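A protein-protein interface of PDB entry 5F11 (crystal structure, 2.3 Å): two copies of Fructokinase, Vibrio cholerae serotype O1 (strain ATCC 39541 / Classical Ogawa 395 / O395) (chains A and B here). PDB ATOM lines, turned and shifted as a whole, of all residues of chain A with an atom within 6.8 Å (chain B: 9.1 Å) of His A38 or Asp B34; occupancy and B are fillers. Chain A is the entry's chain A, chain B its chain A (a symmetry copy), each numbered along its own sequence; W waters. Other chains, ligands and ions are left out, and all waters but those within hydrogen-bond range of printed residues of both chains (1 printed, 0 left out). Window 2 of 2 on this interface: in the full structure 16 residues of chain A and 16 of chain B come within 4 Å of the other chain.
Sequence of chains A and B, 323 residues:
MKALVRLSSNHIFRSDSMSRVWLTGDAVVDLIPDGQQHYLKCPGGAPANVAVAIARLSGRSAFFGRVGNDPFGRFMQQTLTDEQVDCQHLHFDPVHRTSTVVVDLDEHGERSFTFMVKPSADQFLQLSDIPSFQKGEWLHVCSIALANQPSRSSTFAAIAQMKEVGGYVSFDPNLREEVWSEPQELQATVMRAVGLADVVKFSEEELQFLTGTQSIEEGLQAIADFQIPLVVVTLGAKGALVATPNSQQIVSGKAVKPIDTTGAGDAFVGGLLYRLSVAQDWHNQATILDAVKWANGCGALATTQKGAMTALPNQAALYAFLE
The backbone carbonyl oxygen of Gln A37 sits at hydrogen-bond distance from the backbone NH of Lys B41 (3.0 Å).
N of Tyr A39 sits at hydrogen-bond distance from O of Tyr B39.
Water W1 bridges ND1 of His A38 (3.1 Å) and ND1 of His B38 (3.1 Å).
O of Ile A32 is in hydrogen-bond range of N of Leu A40 (2.8 Å).
O of Ile B32 lies within hydrogen-bond range of N of Leu B40 (2.8 Å).
The side-chain carboxylate of Asp B34 is in salt-bridge range of the side-chain amino group of Lys B306 (3.4 Å).
Of chain B, only Asp B34, Tyr B39 and Leu B40 come within 4 Å of His A38.
Asp B34 touches just one residue of chain A: His A38.
Of the printed residues of chain A, Leu B40 touches Gln A37 and His A38.
Printed residues of chain B within 4 Å of Leu A40: Gln B37 and His B38.
Of the printed residues of chain B, Asp A34 touches His B38 (2.9 Å).
Of the printed residues of chain B, Tyr A39 touches His B38, Tyr B39 and Lys B41.
Printed residues of chain B within 4 Å of Gln A37: Leu B40 and Lys B41.
Val B103 touches none of the printed residues of chain A.
Ile B32 touches none of the printed residues of chain A.
The nearest printed residue of chain A that does not touch His B38 is His A38 (4.3 Å).
Of the 18 printed residues of chain B, 6 touch a printed residue of chain A.
Along chain B the printed residues that touch a printed residue of chain A span positions 34 to 41.
Of the 9 printed residues of chain A, 5 touch a printed residue of chain B.
Hydrophobic or aromatic side chains of chain A within 4 Å of the printed part of chain B: His A38, Tyr A39 and Leu A40.
Asp A34 touches His B38, and with the chains exchanged His A38 touches Asp B34.
Gln A37 touches Leu B40, and with the chains exchanged Leu A40 touches Gln B37.
His A38 touches Tyr B39, and with the chains exchanged Tyr A39 touches His B38.
His A38 touches Leu B40, and with the chains exchanged Leu A40 touches His B38.
Positions printed for both chains: 32, 33, 34, 35, 36, 37, 38, 39 and 40.
Of the 11 pairs that touch across the chains among the printed residues, 9 have their exchanged pair printed and touching as well.
Among the printed residues, merely in contact across the chains: Asp A34 with His B38 (2.9 Å), His A38 with Asp B34 (2.9 Å), Tyr A39 with His B38 (3.1 Å), His A38 with Tyr B39 (3.1 Å), His A38 with Leu B40 (3.4 Å), Leu A40 with His B38 (3.4 Å), Tyr A39 with Lys B41 (3.7 Å), Gln A37 with Leu B40 (3.7 Å) and Leu A40 with Gln B37 (3.7 Å).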
ATOM      1  N   ILE A  32       1.562  10.389  22.002  1.00  0.00           N
ATOM      2  CA  ILE A  32       1.532  10.112  20.574  1.00  0.00           C
ATOM      3  C   ILE A  32       1.609   8.609  20.346  1.00  0.00           C
ATOM      4  O   ILE A  32       2.493   7.948  20.883  1.00  0.00           O
ATOM      5  CB  ILE A  32       2.682  10.862  19.854  1.00  0.00           C
ATOM      6  CG1 ILE A  32       2.644  12.351  20.227  1.00  0.00           C
ATOM      7  CG2 ILE A  32       2.626  10.654  18.340  1.00  0.00           C
ATOM      8  CD1 ILE A  32       3.686  13.210  19.534  1.00  0.00           C
ATOM      9  N   PRO A  33       0.656   8.062  19.571  1.00  0.00           N
ATOM     10  CA  PRO A  33       0.544   6.624  19.297  1.00  0.00           C
ATOM     11  C   PRO A  33       1.839   6.035  18.753  1.00  0.00           C
ATOM     12  O   PRO A  33       2.483   6.653  17.909  1.00  0.00           O
ATOM     13  CB  PRO A  33      -0.544   6.558  18.221  1.00  0.00           C
ATOM     14  CG  PRO A  33      -1.360   7.747  18.441  1.00  0.00           C
ATOM     15  CD  PRO A  33      -0.405   8.822  18.888  1.00  0.00           C
ATOM     16  N   ASP A  34       2.213   4.856  19.235  1.00  0.00           N
ATOM     17  CA  ASP A  34       3.416   4.201  18.744  1.00  0.00           C
ATOM     18  C   ASP A  34       3.263   2.688  18.686  1.00  0.00           C
ATOM     19  O   ASP A  34       2.660   2.169  17.745  1.00  0.00           O
ATOM     20  CB  ASP A  34       4.631   4.579  19.589  1.00  0.00           C
ATOM     21  CG  ASP A  34       5.928   4.461  18.819  1.00  0.00           C
ATOM     22  OD1 ASP A  34       6.910   3.953  19.394  1.00  0.00           O
ATOM     23  OD2 ASP A  34       5.963   4.876  17.636  1.00  0.00           O
ATOM     24  N   GLY A  35       3.811   2.005  19.693  1.00  0.00           N
ATOM     25  CA  GLY A  35       3.870   0.551  19.757  1.00  0.00           C
ATOM     26  C   GLY A  35       2.736  -0.187  19.073  1.00  0.00           C
ATOM     27  O   GLY A  35       2.932  -0.772  18.013  1.00  0.00           O
ATOM     28  N   GLN A  36       1.561  -0.153  19.697  1.00  0.00           N
ATOM     29  CA  GLN A  36       0.289  -0.583  19.116  1.00  0.00           C
ATOM     30  C   GLN A  36      -0.776   0.077  19.980  1.00  0.00           C
ATOM     31  O   GLN A  36      -1.614   0.842  19.498  1.00  0.00           O
ATOM     32  CB  GLN A  36       0.115  -2.104  19.156  1.00  0.00           C
ATOM     33  CG  GLN A  36       0.910  -2.911  18.119  1.00  0.00           C
ATOM     34  CD  GLN A  36       0.612  -2.524  16.672  1.00  0.00           C
ATOM     35  OE1 GLN A  36       1.024  -1.467  16.193  1.00  0.00           O
ATOM     36  NE2 GLN A  36      -0.099  -3.396  15.967  1.00  0.00           N
ATOM     37  N   GLN A  37      -0.727  -0.238  21.270  1.00  0.00           N
ATOM     38  CA  GLN A  37      -1.447   0.515  22.285  1.00  0.00           C
ATOM     39  C   GLN A  37      -0.430   1.078  23.265  1.00  0.00           C
ATOM     40  O   GLN A  37      -0.564   0.907  24.478  1.00  0.00           O
ATOM     41  CB  GLN A  37      -2.456  -0.365  23.027  1.00  0.00           C
ATOM     42  CG  GLN A  37      -3.505  -1.018  22.130  1.00  0.00           C
ATOM     43  CD  GLN A  37      -3.151  -2.445  21.741  1.00  0.00           C
ATOM     44  OE1 GLN A  37      -2.260  -3.060  22.326  1.00  0.00           O
ATOM     45  NE2 GLN A  37      -3.852  -2.976  20.747  1.00  0.00           N
ATOM     46  N   HIS A  38       0.602   1.719  22.722  1.00  0.00           N
ATOM     47  CA  HIS A  38       1.566   2.462  23.520  1.00  0.00           C
ATOM     48  C   HIS A  38       1.507   3.941  23.140  1.00  0.00           C
ATOM     49  O   HIS A  38       1.018   4.299  22.062  1.00  0.00           O
ATOM     50  CB  HIS A  38       2.986   1.944  23.287  1.00  0.00           C
ATOM     51  CG  HIS A  38       3.226   0.565  23.811  1.00  0.00           C
ATOM     52  ND1 HIS A  38       4.128   0.298  24.819  1.00  0.00           N
ATOM     53  CD2 HIS A  38       2.689  -0.629  23.459  1.00  0.00           C
ATOM     54  CE1 HIS A  38       4.132  -0.999  25.071  1.00  0.00           C
ATOM     55  NE2 HIS A  38       3.268  -1.584  24.260  1.00  0.00           N
ATOM     56  N   TYR A  39       2.008   4.799  24.016  1.00  0.00           N
ATOM     57  CA  TYR A  39       2.131   6.211  23.704  1.00  0.00           C
ATOM     58  C   TYR A  39       3.587   6.640  23.940  1.00  0.00           C
ATOM     59  O   TYR A  39       4.153   6.357  25.001  1.00  0.00           O
ATOM     60  CB  TYR A  39       1.194   7.041  24.593  1.00  0.00           C
ATOM     61  CG  TYR A  39      -0.270   7.060  24.196  1.00  0.00           C
ATOM     62  CD1 TYR A  39      -0.700   7.734  23.059  1.00  0.00           C
ATOM     63  CD2 TYR A  39      -1.229   6.459  24.997  1.00  0.00           C
ATOM     64  CE1 TYR A  39      -2.035   7.772  22.716  1.00  0.00           C
ATOM     65  CE2 TYR A  39      -2.558   6.488  24.659  1.00  0.00           C
ATOM     66  CZ  TYR A  39      -2.959   7.145  23.520  1.00  0.00           C
ATOM     67  OH  TYR A  39      -4.293   7.169  23.192  1.00  0.00           O
ATOM     68  N   LEU A  40       4.205   7.300  22.961  1.00  0.00           N
ATOM     69  CA  LEU A  40       5.452   7.999  23.235  1.00  0.00           C
ATOM     70  C   LEU A  40       5.083   9.164  24.148  1.00  0.00           C
ATOM     71  O   LEU A  40       4.015   9.766  23.996  1.00  0.00           O
ATOM     72  CB  LEU A  40       6.097   8.515  21.949  1.00  0.00           C
ATOM     73  CG  LEU A  40       6.922   7.538  21.096  1.00  0.00           C
ATOM     74  CD1 LEU A  40       7.067   8.038  19.664  1.00  0.00           C
ATOM     75  CD2 LEU A  40       8.300   7.317  21.702  1.00  0.00           C
ATOM     76  N   ASP B  30      -5.420   4.164  32.434  1.00  0.00           N
ATOM     77  CA  ASP B  30      -4.168   4.129  33.172  1.00  0.00           C
ATOM     78  C   ASP B  30      -2.958   4.164  32.246  1.00  0.00           C
ATOM     79  O   ASP B  30      -2.719   3.238  31.473  1.00  0.00           O
ATOM     80  CB  ASP B  30      -4.096   2.865  34.029  1.00  0.00           C
ATOM     81  CG  ASP B  30      -5.061   2.885  35.191  1.00  0.00           C
ATOM     82  OD1 ASP B  30      -5.332   3.981  35.735  1.00  0.00           O
ATOM     83  OD2 ASP B  30      -5.546   1.794  35.564  1.00  0.00           O
ATOM     84  N   LEU B  31      -2.191   5.239  32.343  1.00  0.00           N
ATOM     85  CA  LEU B  31      -0.946   5.369  31.612  1.00  0.00           C
ATOM     86  C   LEU B  31       0.138   4.738  32.475  1.00  0.00           C
ATOM     87  O   LEU B  31       0.399   5.192  33.588  1.00  0.00           O
ATOM     88  CB  LEU B  31      -0.633   6.845  31.341  1.00  0.00           C
ATOM     89  CG  LEU B  31      -1.192   7.523  30.082  1.00  0.00           C
ATOM     90  CD1 LEU B  31      -2.242   6.692  29.371  1.00  0.00           C
ATOM     91  CD2 LEU B  31      -1.751   8.890  30.409  1.00  0.00           C
ATOM     92  N   ILE B  32       0.754   3.676  31.968  1.00  0.00           N
ATOM     93  CA  ILE B  32       1.694   2.896  32.759  1.00  0.00           C
ATOM     94  C   ILE B  32       3.014   2.780  32.010  1.00  0.00           C
ATOM     95  O   ILE B  32       3.030   2.399  30.844  1.00  0.00           O
ATOM     96  CB  ILE B  32       1.098   1.504  33.091  1.00  0.00           C
ATOM     97  CG1 ILE B  32      -0.293   1.672  33.719  1.00  0.00           C
ATOM     98  CG2 ILE B  32       2.033   0.695  33.991  1.00  0.00           C
ATOM     99  CD1 ILE B  32      -0.960   0.378  34.149  1.00  0.00           C
ATOM    100  N   PRO B  33       4.124   3.145  32.675  1.00  0.00           N
ATOM    101  CA  PRO B  33       5.470   3.154  32.086  1.00  0.00           C
ATOM    102  C   PRO B  33       5.840   1.814  31.466  1.00  0.00           C
ATOM    103  O   PRO B  33       5.561   0.772  32.053  1.00  0.00           O
ATOM    104  CB  PRO B  33       6.375   3.432  33.290  1.00  0.00           C
ATOM    105  CG  PRO B  33       5.533   4.165  34.230  1.00  0.00           C
ATOM    106  CD  PRO B  33       4.152   3.583  34.081  1.00  0.00           C
ATOM    107  N   ASP B  34       6.457   1.844  30.290  1.00  0.00           N
ATOM    108  CA  ASP B  34       6.881   0.612  29.643  1.00  0.00           C
ATOM    109  C   ASP B  34       8.193   0.783  28.890  1.00  0.00           C
ATOM    110  O   ASP B  34       9.260   0.765  29.506  1.00  0.00           O
ATOM    111  CB  ASP B  34       5.797   0.083  28.706  1.00  0.00           C
ATOM    112  CG  ASP B  34       5.893  -1.413  28.502  1.00  0.00           C
ATOM    113  OD1 ASP B  34       5.737  -1.862  27.349  1.00  0.00           O
ATOM    114  OD2 ASP B  34       6.128  -2.141  29.496  1.00  0.00           O
ATOM    115  N   GLY B  35       8.093   0.946  27.569  1.00  0.00           N
ATOM    116  CA  GLY B  35       9.234   1.010  26.666  1.00  0.00           C
ATOM    117  C   GLY B  35      10.510   1.584  27.251  1.00  0.00           C
ATOM    118  O   GLY B  35      11.454   0.847  27.513  1.00  0.00           O
ATOM    119  N   GLN B  36      10.519   2.901  27.442  1.00  0.00           N
ATOM    120  CA  GLN B  36      11.531   3.632  28.205  1.00  0.00           C
ATOM    121  C   GLN B  36      10.878   4.964  28.544  1.00  0.00           C
ATOM    122  O   GLN B  36      10.736   5.334  29.710  1.00  0.00           O
ATOM    123  CB  GLN B  36      12.808   3.875  27.394  1.00  0.00           C
ATOM    124  CG  GLN B  36      13.746   2.673  27.218  1.00  0.00           C
ATOM    125  CD  GLN B  36      14.233   2.069  28.534  1.00  0.00           C
ATOM    126  OE1 GLN B  36      13.483   1.402  29.249  1.00  0.00           O
ATOM    127  NE2 GLN B  36      15.503   2.292  28.847  1.00  0.00           N
ATOM    128  N   GLN B  37      10.484   5.678  27.495  1.00  0.00           N
ATOM    129  CA  GLN B  37       9.578   6.810  27.617  1.00  0.00           C
ATOM    130  C   GLN B  37       8.334   6.509  26.796  1.00  0.00           C
ATOM    131  O   GLN B  37       7.915   7.322  25.970  1.00  0.00           O
ATOM    132  CB  GLN B  37      10.229   8.106  27.126  1.00  0.00           C
ATOM    133  CG  GLN B  37      11.514   8.484  27.857  1.00  0.00           C
ATOM    134  CD  GLN B  37      12.770   8.045  27.120  1.00  0.00           C
ATOM    135  OE1 GLN B  37      12.722   7.683  25.946  1.00  0.00           O
ATOM    136  NE2 GLN B  37      13.901   8.077  27.813  1.00  0.00           N
ATOM    137  N   HIS B  38       7.775   5.321  27.008  1.00  0.00           N
ATOM    138  CA  HIS B  38       6.489   4.951  26.435  1.00  0.00           C
ATOM    139  C   HIS B  38       5.484   4.704  27.559  1.00  0.00           C
ATOM    140  O   HIS B  38       5.867   4.470  28.712  1.00  0.00           O
ATOM    141  CB  HIS B  38       6.611   3.682  25.590  1.00  0.00           C
ATOM    142  CG  HIS B  38       7.410   3.856  24.339  1.00  0.00           C
ATOM    143  ND1 HIS B  38       6.866   3.709  23.081  1.00  0.00           N
ATOM    144  CD2 HIS B  38       8.719   4.156  24.151  1.00  0.00           C
ATOM    145  CE1 HIS B  38       7.800   3.917  22.171  1.00  0.00           C
ATOM    146  NE2 HIS B  38       8.934   4.190  22.794  1.00  0.00           N
ATOM    147  N   TYR B  39       4.202   4.752  27.230  1.00  0.00           N
ATOM    148  CA  TYR B  39       3.164   4.399  28.182  1.00  0.00           C
ATOM    149  C   TYR B  39       2.268   3.321  27.553  1.00  0.00           C
ATOM    150  O   TYR B  39       1.811   3.480  26.418  1.00  0.00           O
ATOM    151  CB  TYR B  39       2.321   5.632  28.538  1.00  0.00           C
ATOM    152  CG  TYR B  39       2.933   6.603  29.531  1.00  0.00           C
ATOM    153  CD1 TYR B  39       3.069   6.269  30.874  1.00  0.00           C
ATOM    154  CD2 TYR B  39       3.311   7.877  29.138  1.00  0.00           C
ATOM    155  CE1 TYR B  39       3.599   7.163  31.780  1.00  0.00           C
ATOM    156  CE2 TYR B  39       3.844   8.769  30.031  1.00  0.00           C
ATOM    157  CZ  TYR B  39       3.987   8.411  31.351  1.00  0.00           C
ATOM    158  OH  TYR B  39       4.521   9.313  32.239  1.00  0.00           O
ATOM    159  N   LEU B  40       2.031   2.221  28.267  1.00  0.00           N
ATOM    160  CA  LEU B  40       0.957   1.322  27.872  1.00  0.00           C
ATOM    161  C   LEU B  40      -0.339   2.085  28.124  1.00  0.00           C
ATOM    162  O   LEU B  40      -0.443   2.841  29.095  1.00  0.00           O
ATOM    163  CB  LEU B  40       0.980   0.031  28.690  1.00  0.00           C
ATOM    164  CG  LEU B  40       1.959  -1.083  28.282  1.00  0.00           C
ATOM    165  CD1 LEU B  40       2.215  -2.046  29.433  1.00  0.00           C
ATOM    166  CD2 LEU B  40       1.435  -1.852  27.077  1.00  0.00           C
ATOM    167  N   LYS B  41      -1.315   1.922  27.240  1.00  0.00           N
ATOM    168  CA  LYS B  41      -2.629   2.502  27.459  1.00  0.00           C
ATOM    169  C   LYS B  41      -3.539   1.390  27.970  1.00  0.00           C
ATOM    170  O   LYS B  41      -3.987   0.537  27.198  1.00  0.00           O
ATOM    171  CB  LYS B  41      -3.170   3.110  26.169  1.00  0.00           C
ATOM    172  CG  LYS B  41      -4.595   3.628  26.263  1.00  0.00           C
ATOM    173  CD  LYS B  41      -5.374   3.215  25.021  1.00  0.00           C
ATOM    174  CE  LYS B  41      -6.273   4.322  24.508  1.00  0.00           C
ATOM    175  NZ  LYS B  41      -6.528   4.143  23.052  1.00  0.00           N
ATOM    176  N   CYS B  42      -3.800   1.396  29.274  1.00  0.00           N
ATOM    177  CA  CYS B  42      -4.500   0.289  29.896  1.00  0.00           C
ATOM    178  C   CYS B  42      -5.871   0.697  30.404  1.00  0.00           C
ATOM    179  O   CYS B  42      -6.033   1.765  30.973  1.00  0.00           O
ATOM    180  CB  CYS B  42      -3.649  -0.305  31.020  1.00  0.00           C
ATOM    181  SG  CYS B  42      -2.088  -1.097  30.448  1.00  0.00           S
ATOM    182  N   VAL B 103       0.708   6.199  36.189  1.00  0.00           N
ATOM    183  CA  VAL B 103       1.226   5.314  37.231  1.00  0.00           C
ATOM    184  C   VAL B 103       2.752   5.403  37.425  1.00  0.00           C
ATOM    185  O   VAL B 103       3.517   5.411  36.468  1.00  0.00           O
ATOM    186  CB  VAL B 103       0.811   3.844  36.984  1.00  0.00           C
ATOM    187  CG1 VAL B 103       1.226   2.965  38.156  1.00  0.00           C
ATOM    188  CG2 VAL B 103      -0.679   3.743  36.774  1.00  0.00           C
ATOM    189  N   LEU B 105       5.512   3.112  38.999  1.00  0.00           N
ATOM    190  CA  LEU B 105       5.716   1.740  39.461  1.00  0.00           C
ATOM    191  C   LEU B 105       6.640   1.633  40.684  1.00  0.00           C
ATOM    192  O   LEU B 105       6.646   0.597  41.368  1.00  0.00           O
ATOM    193  CB  LEU B 105       6.258   0.872  38.325  1.00  0.00           C
ATOM    194  CG  LEU B 105       5.396   0.749  37.068  1.00  0.00           C
ATOM    195  CD1 LEU B 105       6.196   0.131  35.917  1.00  0.00           C
ATOM    196  CD2 LEU B 105       4.145  -0.060  37.356  1.00  0.00           C
ATOM    197  N   ILE B 259       4.281  -8.601  39.547  1.00  0.00           N
ATOM    198  CA  ILE B 259       4.874  -7.803  38.489  1.00  0.00           C
ATOM    199  C   ILE B 259       4.216  -6.423  38.471  1.00  0.00           C
ATOM    200  O   ILE B 259       4.879  -5.409  38.300  1.00  0.00           O
ATOM    201  CB  ILE B 259       4.736  -8.485  37.117  1.00  0.00           C
ATOM    202  CG1 ILE B 259       5.437  -9.843  37.126  1.00  0.00           C
ATOM    203  CG2 ILE B 259       5.329  -7.619  36.027  1.00  0.00           C
ATOM    204  CD1 ILE B 259       5.354 -10.576  35.803  1.00  0.00           C
ATOM    205  N   LYS B 306       0.982  -6.282  33.748  1.00  0.00           N
ATOM    206  CA  LYS B 306       0.718  -4.847  33.846  1.00  0.00           C
ATOM    207  C   LYS B 306      -0.715  -4.559  33.418  1.00  0.00           C
ATOM    208  O   LYS B 306      -1.266  -5.259  32.569  1.00  0.00           O
ATOM    209  CB  LYS B 306       1.695  -4.063  32.974  1.00  0.00           C
ATOM    210  CG  LYS B 306       3.154  -4.264  33.347  1.00  0.00           C
ATOM    211  CD  LYS B 306       4.061  -3.316  32.575  1.00  0.00           C
ATOM    212  CE  LYS B 306       5.337  -3.025  33.359  1.00  0.00           C
ATOM    213  NZ  LYS B 306       6.051  -1.826  32.839  1.00  0.00           N
ATOM    214  N   GLY B 307      -1.326  -3.547  34.023  1.00  0.00           N
ATOM    215  CA  GLY B 307      -2.714  -3.242  33.744  1.00  0.00           C
ATOM    216  C   GLY B 307      -3.633  -3.927  34.736  1.00  0.00           C
ATOM    217  O   GLY B 307      -3.546  -5.141  34.945  1.00  0.00           O
HETATM  218  O   HOH W   1       6.677   0.636  23.124  1.00  0.00           O
